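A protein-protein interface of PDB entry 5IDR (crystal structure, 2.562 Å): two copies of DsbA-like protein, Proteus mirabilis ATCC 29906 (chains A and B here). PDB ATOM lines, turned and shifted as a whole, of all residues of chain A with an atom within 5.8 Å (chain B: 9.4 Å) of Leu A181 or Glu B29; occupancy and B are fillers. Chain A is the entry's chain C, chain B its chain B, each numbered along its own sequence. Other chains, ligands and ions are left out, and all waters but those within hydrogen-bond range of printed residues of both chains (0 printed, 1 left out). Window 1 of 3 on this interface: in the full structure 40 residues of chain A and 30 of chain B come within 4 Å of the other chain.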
ATOM      1  N   LEU A  35       1.645  -0.444 -29.621  1.00  0.00           N
ATOM      2  CA  LEU A  35       1.818  -1.368 -28.513  1.00  0.00           C
ATOM      3  C   LEU A  35       1.150  -0.843 -27.236  1.00  0.00           C
ATOM      4  O   LEU A  35       0.569  -1.611 -26.474  1.00  0.00           O
ATOM      5  CB  LEU A  35       3.301  -1.616 -28.286  1.00  0.00           C
ATOM      6  CG  LEU A  35       3.710  -2.590 -27.191  1.00  0.00           C
ATOM      7  CD1 LEU A  35       2.853  -3.840 -27.167  1.00  0.00           C
ATOM      8  CD2 LEU A  35       5.165  -2.958 -27.434  1.00  0.00           C
ATOM      9  N   LYS A  38      -2.426  -1.553 -27.252  1.00  0.00           N
ATOM     10  CA  LYS A  38      -2.543  -3.003 -27.066  1.00  0.00           C
ATOM     11  C   LYS A  38      -2.512  -3.349 -25.581  1.00  0.00           C
ATOM     12  O   LYS A  38      -3.384  -4.056 -25.079  1.00  0.00           O
ATOM     13  CB  LYS A  38      -1.417  -3.732 -27.800  1.00  0.00           C
ATOM     14  CG  LYS A  38      -1.598  -5.255 -27.908  1.00  0.00           C
ATOM     15  CD  LYS A  38      -0.248  -5.954 -28.173  1.00  0.00           C
ATOM     16  CE  LYS A  38      -0.398  -7.394 -28.601  1.00  0.00           C
ATOM     17  NZ  LYS A  38      -0.832  -8.274 -27.488  1.00  0.00           N
ATOM     18  N   LYS A  39      -1.507  -2.842 -24.875  1.00  0.00           N
ATOM     19  CA  LYS A  39      -1.410  -3.068 -23.435  1.00  0.00           C
ATOM     20  C   LYS A  39      -2.604  -2.474 -22.701  1.00  0.00           C
ATOM     21  O   LYS A  39      -3.024  -2.996 -21.669  1.00  0.00           O
ATOM     22  CB  LYS A  39      -0.119  -2.475 -22.864  1.00  0.00           C
ATOM     23  CG  LYS A  39       1.152  -3.029 -23.476  1.00  0.00           C
ATOM     24  CD  LYS A  39       2.326  -2.852 -22.546  1.00  0.00           C
ATOM     25  CE  LYS A  39       3.532  -2.314 -23.284  1.00  0.00           C
ATOM     26  NZ  LYS A  39       4.718  -2.236 -22.391  1.00  0.00           N
ATOM     27  N   GLU A  42      -5.665  -4.732 -22.988  1.00  0.00           N
ATOM     28  CA  GLU A  42      -5.562  -5.995 -22.271  1.00  0.00           C
ATOM     29  C   GLU A  42      -5.627  -5.881 -20.749  1.00  0.00           C
ATOM     30  O   GLU A  42      -6.286  -6.686 -20.102  1.00  0.00           O
ATOM     31  CB  GLU A  42      -4.273  -6.693 -22.693  1.00  0.00           C
ATOM     32  CG  GLU A  42      -4.298  -7.048 -24.172  1.00  0.00           C
ATOM     33  CD  GLU A  42      -2.984  -7.588 -24.694  1.00  0.00           C
ATOM     34  OE1 GLU A  42      -2.013  -7.683 -23.909  1.00  0.00           O
ATOM     35  OE2 GLU A  42      -2.933  -7.916 -25.900  1.00  0.00           O
ATOM     36  N   LEU A 111       7.523 -16.930 -17.319  1.00  0.00           N
ATOM     37  CA  LEU A 111       7.503 -15.485 -17.547  1.00  0.00           C
ATOM     38  C   LEU A 111       8.909 -14.912 -17.435  1.00  0.00           C
ATOM     39  O   LEU A 111       9.742 -15.455 -16.722  1.00  0.00           O
ATOM     40  CB  LEU A 111       6.552 -14.796 -16.556  1.00  0.00           C
ATOM     41  CG  LEU A 111       5.067 -15.024 -16.860  1.00  0.00           C
ATOM     42  CD1 LEU A 111       4.189 -14.678 -15.668  1.00  0.00           C
ATOM     43  CD2 LEU A 111       4.628 -14.212 -18.081  1.00  0.00           C
ATOM     44  N   PRO A 112       9.178 -13.805 -18.142  1.00  0.00           N
ATOM     45  CA  PRO A 112      10.523 -13.222 -18.161  1.00  0.00           C
ATOM     46  C   PRO A 112      10.754 -12.061 -17.172  1.00  0.00           C
ATOM     47  O   PRO A 112      11.615 -11.216 -17.428  1.00  0.00           O
ATOM     48  CB  PRO A 112      10.626 -12.725 -19.596  1.00  0.00           C
ATOM     49  CG  PRO A 112       9.247 -12.252 -19.897  1.00  0.00           C
ATOM     50  CD  PRO A 112       8.307 -13.159 -19.141  1.00  0.00           C
ATOM     51  N   PHE A 113      10.036 -12.025 -16.051  1.00  0.00           N
ATOM     52  CA  PHE A 113       9.983 -10.801 -15.256  1.00  0.00           C
ATOM     53  C   PHE A 113      11.299 -10.523 -14.562  1.00  0.00           C
ATOM     54  O   PHE A 113      11.622  -9.367 -14.309  1.00  0.00           O
ATOM     55  CB  PHE A 113       8.852 -10.856 -14.222  1.00  0.00           C
ATOM     56  CG  PHE A 113       7.463 -10.813 -14.825  1.00  0.00           C
ATOM     57  CD1 PHE A 113       7.252 -10.368 -16.123  1.00  0.00           C
ATOM     58  CD2 PHE A 113       6.358 -11.218 -14.077  1.00  0.00           C
ATOM     59  CE1 PHE A 113       5.956 -10.349 -16.667  1.00  0.00           C
ATOM     60  CE2 PHE A 113       5.070 -11.198 -14.614  1.00  0.00           C
ATOM     61  CZ  PHE A 113       4.870 -10.771 -15.905  1.00  0.00           C
ATOM     62  N   THR A 176       5.640 -17.804 -27.989  1.00  0.00           N
ATOM     63  CA  THR A 176       4.897 -18.407 -26.884  1.00  0.00           C
ATOM     64  C   THR A 176       5.177 -17.654 -25.591  1.00  0.00           C
ATOM     65  O   THR A 176       4.307 -17.507 -24.734  1.00  0.00           O
ATOM     66  CB  THR A 176       5.279 -19.911 -26.720  1.00  0.00           C
ATOM     67  OG1 THR A 176       4.791 -20.658 -27.846  1.00  0.00           O
ATOM     68  CG2 THR A 176       4.722 -20.519 -25.422  1.00  0.00           C
ATOM     69  N   LEU A 177       6.405 -17.177 -25.449  1.00  0.00           N
ATOM     70  CA  LEU A 177       6.801 -16.482 -24.236  1.00  0.00           C
ATOM     71  C   LEU A 177       6.071 -15.127 -24.175  1.00  0.00           C
ATOM     72  O   LEU A 177       5.657 -14.674 -23.103  1.00  0.00           O
ATOM     73  CB  LEU A 177       8.325 -16.317 -24.188  1.00  0.00           C
ATOM     74  CG  LEU A 177       8.892 -15.567 -22.982  1.00  0.00           C
ATOM     75  CD1 LEU A 177       8.314 -16.098 -21.694  1.00  0.00           C
ATOM     76  CD2 LEU A 177      10.401 -15.685 -22.945  1.00  0.00           C
ATOM     77  N   GLN A 178       5.895 -14.509 -25.341  1.00  0.00           N
ATOM     78  CA  GLN A 178       5.132 -13.271 -25.463  1.00  0.00           C
ATOM     79  C   GLN A 178       3.632 -13.509 -25.307  1.00  0.00           C
ATOM     80  O   GLN A 178       2.897 -12.600 -24.950  1.00  0.00           O
ATOM     81  CB  GLN A 178       5.423 -12.604 -26.807  1.00  0.00           C
ATOM     82  CG  GLN A 178       4.751 -11.264 -27.004  1.00  0.00           C
ATOM     83  CD  GLN A 178       3.377 -11.381 -27.617  1.00  0.00           C
ATOM     84  OE1 GLN A 178       3.062 -12.359 -28.303  1.00  0.00           O
ATOM     85  NE2 GLN A 178       2.541 -10.377 -27.371  1.00  0.00           N
ATOM     86  N   ASN A 179       3.163 -14.725 -25.567  1.00  0.00           N
ATOM     87  CA  ASN A 179       1.743 -15.003 -25.376  1.00  0.00           C
ATOM     88  C   ASN A 179       1.427 -15.077 -23.884  1.00  0.00           C
ATOM     89  O   ASN A 179       0.344 -14.674 -23.444  1.00  0.00           O
ATOM     90  CB  ASN A 179       1.326 -16.301 -26.067  1.00  0.00           C
ATOM     91  CG  ASN A 179       1.267 -16.178 -27.585  1.00  0.00           C
ATOM     92  OD1 ASN A 179       1.172 -15.088 -28.148  1.00  0.00           O
ATOM     93  ND2 ASN A 179       1.322 -17.315 -28.253  1.00  0.00           N
ATOM     94  N   ASN A 180       2.389 -15.583 -23.118  1.00  0.00           N
ATOM     95  CA  ASN A 180       2.278 -15.663 -21.670  1.00  0.00           C
ATOM     96  C   ASN A 180       2.259 -14.273 -21.040  1.00  0.00           C
ATOM     97  O   ASN A 180       1.612 -14.032 -20.011  1.00  0.00           O
ATOM     98  CB  ASN A 180       3.439 -16.465 -21.106  1.00  0.00           C
ATOM     99  CG  ASN A 180       3.338 -17.933 -21.421  1.00  0.00           C
ATOM    100  OD1 ASN A 180       2.396 -18.382 -22.077  1.00  0.00           O
ATOM    101  ND2 ASN A 180       4.308 -18.696 -20.945  1.00  0.00           N
ATOM    102  N   LEU A 181       2.993 -13.365 -21.664  1.00  0.00           N
ATOM    103  CA  LEU A 181       2.998 -11.978 -21.245  1.00  0.00           C
ATOM    104  C   LEU A 181       1.612 -11.377 -21.463  1.00  0.00           C
ATOM    105  O   LEU A 181       1.042 -10.783 -20.547  1.00  0.00           O
ATOM    106  CB  LEU A 181       4.057 -11.211 -22.024  1.00  0.00           C
ATOM    107  CG  LEU A 181       4.837 -10.104 -21.339  1.00  0.00           C
ATOM    108  CD1 LEU A 181       5.489 -10.594 -20.072  1.00  0.00           C
ATOM    109  CD2 LEU A 181       5.883  -9.614 -22.317  1.00  0.00           C
ATOM    110  N   GLU A 182       1.078 -11.538 -22.677  1.00  0.00           N
ATOM    111  CA  GLU A 182      -0.297 -11.139 -22.990  1.00  0.00           C
ATOM    112  C   GLU A 182      -1.276 -11.718 -21.989  1.00  0.00           C
ATOM    113  O   GLU A 182      -2.150 -11.028 -21.483  1.00  0.00           O
ATOM    114  CB  GLU A 182      -0.722 -11.607 -24.392  1.00  0.00           C
ATOM    115  CG  GLU A 182      -0.313 -10.726 -25.555  1.00  0.00           C
ATOM    116  CD  GLU A 182      -0.587 -11.388 -26.892  1.00  0.00           C
ATOM    117  OE1 GLU A 182      -1.538 -12.196 -26.969  1.00  0.00           O
ATOM    118  OE2 GLU A 182       0.155 -11.116 -27.862  1.00  0.00           O
ATOM    119  N   LEU A 183      -1.142 -13.005 -21.726  1.00  0.00           N
ATOM    120  CA  LEU A 183      -2.093 -13.682 -20.871  1.00  0.00           C
ATOM    121  C   LEU A 183      -2.074 -13.067 -19.487  1.00  0.00           C
ATOM    122  O   LEU A 183      -3.123 -12.744 -18.934  1.00  0.00           O
ATOM    123  CB  LEU A 183      -1.787 -15.176 -20.803  1.00  0.00           C
ATOM    124  CG  LEU A 183      -2.812 -16.028 -20.047  1.00  0.00           C
ATOM    125  CD1 LEU A 183      -4.201 -15.906 -20.678  1.00  0.00           C
ATOM    126  CD2 LEU A 183      -2.384 -17.493 -19.995  1.00  0.00           C
ATOM    127  N   SER A 184      -0.883 -12.889 -18.927  1.00  0.00           N
ATOM    128  CA  SER A 184      -0.768 -12.381 -17.566  1.00  0.00           C
ATOM    129  C   SER A 184      -1.303 -10.941 -17.452  1.00  0.00           C
ATOM    130  O   SER A 184      -1.861 -10.563 -16.427  1.00  0.00           O
ATOM    131  CB  SER A 184       0.686 -12.477 -17.094  1.00  0.00           C
ATOM    132  OG  SER A 184       1.518 -11.593 -17.815  1.00  0.00           O
ATOM    133  N   ARG A 185      -1.148 -10.139 -18.504  1.00  0.00           N
ATOM    134  CA  ARG A 185      -1.769  -8.813 -18.537  1.00  0.00           C
ATOM    135  C   ARG A 185      -3.283  -8.874 -18.392  1.00  0.00           C
ATOM    136  O   ARG A 185      -3.860  -8.176 -17.560  1.00  0.00           O
ATOM    137  CB  ARG A 185      -1.441  -8.086 -19.838  1.00  0.00           C
ATOM    138  CG  ARG A 185      -0.250  -7.173 -19.760  1.00  0.00           C
ATOM    139  CD  ARG A 185      -0.284  -6.169 -20.874  1.00  0.00           C
ATOM    140  NE  ARG A 185      -0.118  -6.784 -22.189  1.00  0.00           N
ATOM    141  CZ  ARG A 185       1.054  -7.036 -22.766  1.00  0.00           C
ATOM    142  NH1 ARG A 185       2.188  -6.748 -22.146  1.00  0.00           N
ATOM    143  NH2 ARG A 185       1.089  -7.589 -23.969  1.00  0.00           N
ATOM    144  N   LYS A 186      -3.925  -9.693 -19.221  1.00  0.00           N
ATOM    145  CA  LYS A 186      -5.378  -9.832 -19.199  1.00  0.00           C
ATOM    146  C   LYS A 186      -5.902 -10.367 -17.882  1.00  0.00           C
ATOM    147  O   LYS A 186      -7.042 -10.104 -17.532  1.00  0.00           O
ATOM    148  CB  LYS A 186      -5.843 -10.743 -20.327  1.00  0.00           C
ATOM    149  CG  LYS A 186      -5.464 -10.219 -21.694  1.00  0.00           C
ATOM    150  CD  LYS A 186      -5.932 -11.118 -22.816  1.00  0.00           C
ATOM    151  CE  LYS A 186      -5.264 -10.713 -24.134  1.00  0.00           C
ATOM    152  NZ  LYS A 186      -5.579 -11.639 -25.265  1.00  0.00           N
ATOM    153  N   LEU B  21       4.585  -3.451 -38.703  1.00  0.00           N
ATOM    154  CA  LEU B  21       4.878  -3.229 -37.297  1.00  0.00           C
ATOM    155  C   LEU B  21       3.733  -2.555 -36.558  1.00  0.00           C
ATOM    156  O   LEU B  21       3.349  -2.996 -35.482  1.00  0.00           O
ATOM    157  CB  LEU B  21       6.133  -2.388 -37.139  1.00  0.00           C
ATOM    158  CG  LEU B  21       7.397  -3.201 -36.929  1.00  0.00           C
ATOM    159  CD1 LEU B  21       8.573  -2.267 -36.983  1.00  0.00           C
ATOM    160  CD2 LEU B  21       7.359  -3.961 -35.602  1.00  0.00           C
ATOM    161  N   ASN B  24       0.613  -4.915 -36.142  1.00  0.00           N
ATOM    162  CA  ASN B  24       0.816  -6.083 -35.281  1.00  0.00           C
ATOM    163  C   ASN B  24       1.864  -5.835 -34.194  1.00  0.00           C
ATOM    164  O   ASN B  24       2.995  -6.309 -34.293  1.00  0.00           O
ATOM    165  CB  ASN B  24       1.230  -7.291 -36.125  1.00  0.00           C
ATOM    166  CG  ASN B  24       0.249  -7.583 -37.232  1.00  0.00           C
ATOM    167  OD1 ASN B  24       0.259  -6.927 -38.276  1.00  0.00           O
ATOM    168  ND2 ASN B  24      -0.611  -8.571 -37.015  1.00  0.00           N
ATOM    169  N   PRO B  25       1.487  -5.089 -33.146  1.00  0.00           N
ATOM    170  CA  PRO B  25       2.434  -4.765 -32.076  1.00  0.00           C
ATOM    171  C   PRO B  25       2.940  -5.985 -31.323  1.00  0.00           C
ATOM    172  O   PRO B  25       3.875  -5.850 -30.533  1.00  0.00           O
ATOM    173  CB  PRO B  25       1.619  -3.870 -31.146  1.00  0.00           C
ATOM    174  CG  PRO B  25       0.483  -3.386 -31.977  1.00  0.00           C
ATOM    175  CD  PRO B  25       0.186  -4.432 -32.950  1.00  0.00           C
ATOM    176  N   GLU B  26       2.342  -7.150 -31.542  1.00  0.00           N
ATOM    177  CA  GLU B  26       2.895  -8.361 -30.945  1.00  0.00           C
ATOM    178  C   GLU B  26       4.246  -8.653 -31.595  1.00  0.00           C
ATOM    179  O   GLU B  26       5.137  -9.222 -30.963  1.00  0.00           O
ATOM    180  CB  GLU B  26       1.947  -9.556 -31.090  1.00  0.00           C
ATOM    181  CG  GLU B  26       1.559  -9.900 -32.514  1.00  0.00           C
ATOM    182  CD  GLU B  26       0.887 -11.252 -32.606  1.00  0.00           C
ATOM    183  OE1 GLU B  26       0.501 -11.798 -31.545  1.00  0.00           O
ATOM    184  OE2 GLU B  26       0.758 -11.775 -33.735  1.00  0.00           O
ATOM    185  N   ILE B  27       4.400  -8.247 -32.854  1.00  0.00           N
ATOM    186  CA  ILE B  27       5.687  -8.374 -33.530  1.00  0.00           C
ATOM    187  C   ILE B  27       6.716  -7.579 -32.754  1.00  0.00           C
ATOM    188  O   ILE B  27       7.816  -8.058 -32.477  1.00  0.00           O
ATOM    189  CB  ILE B  27       5.652  -7.872 -34.987  1.00  0.00           C
ATOM    190  CG1 ILE B  27       4.792  -8.798 -35.843  1.00  0.00           C
ATOM    191  CG2 ILE B  27       7.064  -7.832 -35.564  1.00  0.00           C
ATOM    192  CD1 ILE B  27       4.677  -8.396 -37.298  1.00  0.00           C
ATOM    193  N   LEU B  28       6.348  -6.352 -32.411  1.00  0.00           N
ATOM    194  CA  LEU B  28       7.232  -5.494 -31.650  1.00  0.00           C
ATOM    195  C   LEU B  28       7.487  -6.105 -30.285  1.00  0.00           C
ATOM    196  O   LEU B  28       8.615  -6.095 -29.811  1.00  0.00           O
ATOM    197  CB  LEU B  28       6.650  -4.082 -31.506  1.00  0.00           C
ATOM    198  CG  LEU B  28       7.414  -3.113 -30.591  1.00  0.00           C
ATOM    199  CD1 LEU B  28       8.861  -2.950 -31.042  1.00  0.00           C
ATOM    200  CD2 LEU B  28       6.697  -1.778 -30.554  1.00  0.00           C
ATOM    201  N   GLU B  29       6.453  -6.649 -29.649  1.00  0.00           N
ATOM    202  CA  GLU B  29       6.630  -7.123 -28.284  1.00  0.00           C
ATOM    203  C   GLU B  29       7.483  -8.391 -28.248  1.00  0.00           C
ATOM    204  O   GLU B  29       8.214  -8.614 -27.281  1.00  0.00           O
ATOM    205  CB  GLU B  29       5.288  -7.372 -27.601  1.00  0.00           C
ATOM    206  CG  GLU B  29       5.448  -7.576 -26.101  1.00  0.00           C
ATOM    207  CD  GLU B  29       4.164  -7.370 -25.342  1.00  0.00           C
ATOM    208  OE1 GLU B  29       4.241  -7.084 -24.132  1.00  0.00           O
ATOM    209  OE2 GLU B  29       3.082  -7.494 -25.955  1.00  0.00           O
ATOM    210  N   GLU B  30       7.396  -9.203 -29.302  1.00  0.00           N
ATOM    211  CA  GLU B  30       8.243 -10.394 -29.434  1.00  0.00           C
ATOM    212  C   GLU B  30       9.684 -10.002 -29.709  1.00  0.00           C
ATOM    213  O   GLU B  30      10.613 -10.569 -29.131  1.00  0.00           O
ATOM    214  CB  GLU B  30       7.744 -11.299 -30.552  1.00  0.00           C
ATOM    215  CG  GLU B  30       6.504 -12.072 -30.192  1.00  0.00           C
ATOM    216  CD  GLU B  30       5.755 -12.559 -31.411  1.00  0.00           C
ATOM    217  OE1 GLU B  30       6.411 -12.833 -32.444  1.00  0.00           O
ATOM    218  OE2 GLU B  30       4.512 -12.651 -31.330  1.00  0.00           O
ATOM    219  N   ALA B  31       9.863  -9.034 -30.601  1.00  0.00           N
ATOM    220  CA  ALA B  31      11.182  -8.474 -30.854  1.00  0.00           C
ATOM    221  C   ALA B  31      11.784  -7.936 -29.551  1.00  0.00           C
ATOM    222  O   ALA B  31      12.994  -8.014 -29.327  1.00  0.00           O
ATOM    223  CB  ALA B  31      11.093  -7.384 -31.900  1.00  0.00           C
ATOM    224  N   ILE B  32      10.926  -7.400 -28.689  1.00  0.00           N
ATOM    225  CA  ILE B  32      11.351  -6.897 -27.385  1.00  0.00           C
ATOM    226  C   ILE B  32      11.713  -8.054 -26.486  1.00  0.00           C
ATOM    227  O   ILE B  32      12.665  -7.973 -25.711  1.00  0.00           O
ATOM    228  CB  ILE B  32      10.261  -6.056 -26.707  1.00  0.00           C
ATOM    229  CG1 ILE B  32      10.075  -4.743 -27.451  1.00  0.00           C
ATOM    230  CG2 ILE B  32      10.635  -5.744 -25.264  1.00  0.00           C
ATOM    231  CD1 ILE B  32       8.828  -4.007 -27.047  1.00  0.00           C
ATOM    232  N   MET B  33      10.924  -9.120 -26.573  1.00  0.00           N
ATOM    233  CA  MET B  33      11.237 -10.362 -25.882  1.00  0.00           C
ATOM    234  C   MET B  33      12.563 -10.932 -26.381  1.00  0.00           C
ATOM    235  O   MET B  33      13.344 -11.459 -25.603  1.00  0.00           O
ATOM    236  CB  MET B  33      10.116 -11.394 -26.078  1.00  0.00           C
ATOM    237  CG  MET B  33       8.920 -11.233 -25.146  1.00  0.00           C
ATOM    238  SD  MET B  33       9.345 -11.177 -23.398  1.00  0.00           S
ATOM    239  CE  MET B  33      10.599 -12.445 -23.328  1.00  0.00           C
ATOM    240  N   ALA B  34      12.818 -10.830 -27.679  1.00  0.00           N
ATOM    241  CA  ALA B  34      14.067 -11.330 -28.233  1.00  0.00           C
ATOM    242  C   ALA B  34      15.242 -10.505 -27.714  1.00  0.00           C
ATOM    243  O   ALA B  34      16.298 -11.054 -27.385  1.00  0.00           O
ATOM    244  CB  ALA B  34      14.031 -11.312 -29.763  1.00  0.00           C
ATOM    245  N   LEU B  35      15.058  -9.188 -27.645  1.00  0.00           N
ATOM    246  CA  LEU B  35      16.097  -8.301 -27.138  1.00  0.00           C
ATOM    247  C   LEU B  35      16.322  -8.534 -25.639  1.00  0.00           C
ATOM    248  O   LEU B  35      17.431  -8.358 -25.132  1.00  0.00           O
ATOM    249  CB  LEU B  35      15.723  -6.843 -27.414  1.00  0.00           C
ATOM    250  CG  LEU B  35      16.756  -5.764 -27.051  1.00  0.00           C
ATOM    251  CD1 LEU B  35      18.160  -6.130 -27.535  1.00  0.00           C
ATOM    252  CD2 LEU B  35      16.332  -4.413 -27.624  1.00  0.00           C
ATOM    253  N   GLN B  36      15.267  -8.944 -24.940  1.00  0.00           N
ATOM    254  CA  GLN B  36      15.364  -9.280 -23.526  1.00  0.00           C
ATOM    255  C   GLN B  36      16.368 -10.419 -23.286  1.00  0.00           C
ATOM    256  O   GLN B  36      17.042 -10.443 -22.260  1.00  0.00           O
ATOM    257  CB  GLN B  36      13.976  -9.653 -22.986  1.00  0.00           C
ATOM    258  CG  GLN B  36      13.924 -10.119 -21.525  1.00  0.00           C
ATOM    259  CD  GLN B  36      13.820  -8.977 -20.545  1.00  0.00           C
ATOM    260  OE1 GLN B  36      14.406  -7.908 -20.747  1.00  0.00           O
ATOM    261  NE2 GLN B  36      13.060  -9.192 -19.472  1.00  0.00           N
ATOM    262  N   THR B  37      16.474 -11.353 -24.232  1.00  0.00           N
ATOM    263  CA  THR B  37      17.391 -12.488 -24.084  1.00  0.00           C
ATOM    264  C   THR B  37      18.839 -12.086 -24.307  1.00  0.00           C
ATOM    265  O   THR B  37      19.753 -12.842 -23.978  1.00  0.00           O
ATOM    266  CB  THR B  37      17.080 -13.646 -25.069  1.00  0.00           C
ATOM    267  OG1 THR B  37      16.980 -13.138 -26.403  1.00  0.00           O
ATOM    268  CG2 THR B  37      15.797 -14.364 -24.699  1.00  0.00           C
ATOM    269  N   PRO B  85       5.740  -5.305 -13.808  1.00  0.00           N
ATOM    270  CA  PRO B  85       6.359  -6.552 -13.330  1.00  0.00           C
ATOM    271  C   PRO B  85       7.886  -6.534 -13.306  1.00  0.00           C
ATOM    272  O   PRO B  85       8.483  -7.100 -12.389  1.00  0.00           O
ATOM    273  CB  PRO B  85       5.859  -7.598 -14.330  1.00  0.00           C
ATOM    274  CG  PRO B  85       5.484  -6.833 -15.526  1.00  0.00           C
ATOM    275  CD  PRO B  85       4.927  -5.544 -15.011  1.00  0.00           C
ATOM    276  N   TYR B  86       8.511  -5.893 -14.286  1.00  0.00           N
ATOM    277  CA  TYR B  86       9.973  -5.809 -14.307  1.00  0.00           C
ATOM    278  C   TYR B  86      10.446  -4.884 -13.208  1.00  0.00           C
ATOM    279  O   TYR B  86      11.524  -5.088 -12.652  1.00  0.00           O
ATOM    280  CB  TYR B  86      10.490  -5.331 -15.662  1.00  0.00           C
ATOM    281  CG  TYR B  86       9.951  -6.139 -16.817  1.00  0.00           C
ATOM    282  CD1 TYR B  86      10.446  -7.408 -17.094  1.00  0.00           C
ATOM    283  CD2 TYR B  86       8.939  -5.641 -17.618  1.00  0.00           C
ATOM    284  CE1 TYR B  86       9.950  -8.153 -18.138  1.00  0.00           C
ATOM    285  CE2 TYR B  86       8.438  -6.374 -18.665  1.00  0.00           C
ATOM    286  CZ  TYR B  86       8.944  -7.629 -18.922  1.00  0.00           C
ATOM    287  OH  TYR B  86       8.429  -8.353 -19.975  1.00  0.00           O
ATOM    288  N   LYS B 114       0.639   2.560 -15.638  1.00  0.00           N
ATOM    289  CA  LYS B 114      -0.269   1.418 -15.758  1.00  0.00           C
ATOM    290  C   LYS B 114      -1.654   1.674 -15.160  1.00  0.00           C
ATOM    291  O   LYS B 114      -2.434   0.743 -14.949  1.00  0.00           O
ATOM    292  CB  LYS B 114       0.381   0.174 -15.134  1.00  0.00           C
ATOM    293  CG  LYS B 114       1.477  -0.423 -16.049  1.00  0.00           C
ATOM    294  CD  LYS B 114       1.640  -1.925 -15.904  1.00  0.00           C
ATOM    295  CE  LYS B 114       2.459  -2.516 -17.047  1.00  0.00           C
ATOM    296  NZ  LYS B 114       1.737  -2.468 -18.355  1.00  0.00           N
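The guanidinium group of Arg A185 is in salt-bridge range of the side-chain carboxylate of Glu B29.
NE2 of Gln B36 is in hydrogen-bond range of O of Pro A112, 3.2 Å away.
The side-chain amide nitrogen (NE2) of Gln A178 lies within hydrogen-bond range of the side-chain carboxylate (OE2) of Glu B29.
OE1 of Gln A178 sits close to OE2 of Glu B30 (3.4 Å).
The side-chain amide nitrogen (NE2) of Gln A178 sits at hydrogen-bond distance from the side-chain carboxylate (OE2) of Glu A182, at 2.5 Å.
O of Leu A181 is in hydrogen-bond range of OG of Ser A184, at 2.9 Å.
NE of Arg A185 is in salt-bridge range of OE1 of Glu A42.
The side-chain amino group of Lys A38 is in salt-bridge range of the side-chain carboxylate of Glu A182 (3.0 Å).
OE1 of Gln A178 sits close to OD1 of Asn A179 (3.3 Å).
Among the printed residues, pairs that only touch across the chains: Leu A35 with Pro B25 (3.6 Å), Leu A35 with Leu B28 (3.7 Å), Leu A35 with Glu B29 (3.9 Å), Leu A35 with Ile B32 (3.8 Å), Pro A112 with Met B33 (3.7 Å), Pro A112 with Tyr B86 (3.6 Å), Phe A113 with Pro B85 (3.6 Å), Phe A113 with Tyr B86 (3.6 Å), Leu A177 with Met B33 (3.3 Å), Gln A178 with Glu B26 (3.9 Å), Leu A181 with Glu B29 (3.5 Å), Leu A181 with Met B33 (3.9 Å), Leu A181 with Tyr B86 (3.7 Å) and Glu A182 with Glu B26 (3.8 Å).
Of the printed residues of chain B, Leu A35 touches Pro B25 (3.6 Å), Leu B28 (3.7 Å), Glu B29 (3.9 Å) and Ile B32 (3.8 Å).
Printed residues of chain B within 4 Å of Phe A113: Pro B85 (3.6 Å) and Tyr B86 (3.6 Å).
Of the printed residues of chain B, Leu A177 touches Met B33 (3.3 Å).
Printed residues of chain B within 4 Å of Gln A178: Glu B26 (3.9 Å), Glu B29 (3.3 Å) and Glu B30 (3.4 Å).
Leu A181 touches just these residues of chain B: Glu B29, Met B33 and Tyr B86.
No residue of chain B comes within 4 Å of Ser A184.
Of chain A, only Leu A35, Gln A178, Leu A181 and Arg A185 come within 4 Å of Glu B29.
Printed residues of chain A within 4 Å of Gln B36: Pro A112 (3.2 Å).
The nearest residue of chain B that does not touch Leu A181 is Pro B85 (5.9 Å).
The nearest residue of chain A that does not touch Glu B29 is Lys A38 (4.3 Å).
The nearest printed residue of chain A that does not touch Pro B25 is Lys A38 (4.1 Å).
Of the 18 printed residues of chain A, 8 touch a printed residue of chain B.
Hydrophobic or aromatic side chains of chain A within 4 Å of the printed part of chain B: Leu A35, Pro A112, Phe A113, Leu A177 and Leu A181.
Among the printed residues, 18 pairs touch across the chains.
Among the printed residues, Asp or Glu carboxylates within 4 Å of a Lys or Arg side-chain nitrogen of the other chain: Arg A185 with Glu B29 (2.8 Å).
Position printed for both chains: 35.
Of the 18 pairs that touch across the chains among the printed residues, none has its exchanged pair printed and touching as well.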
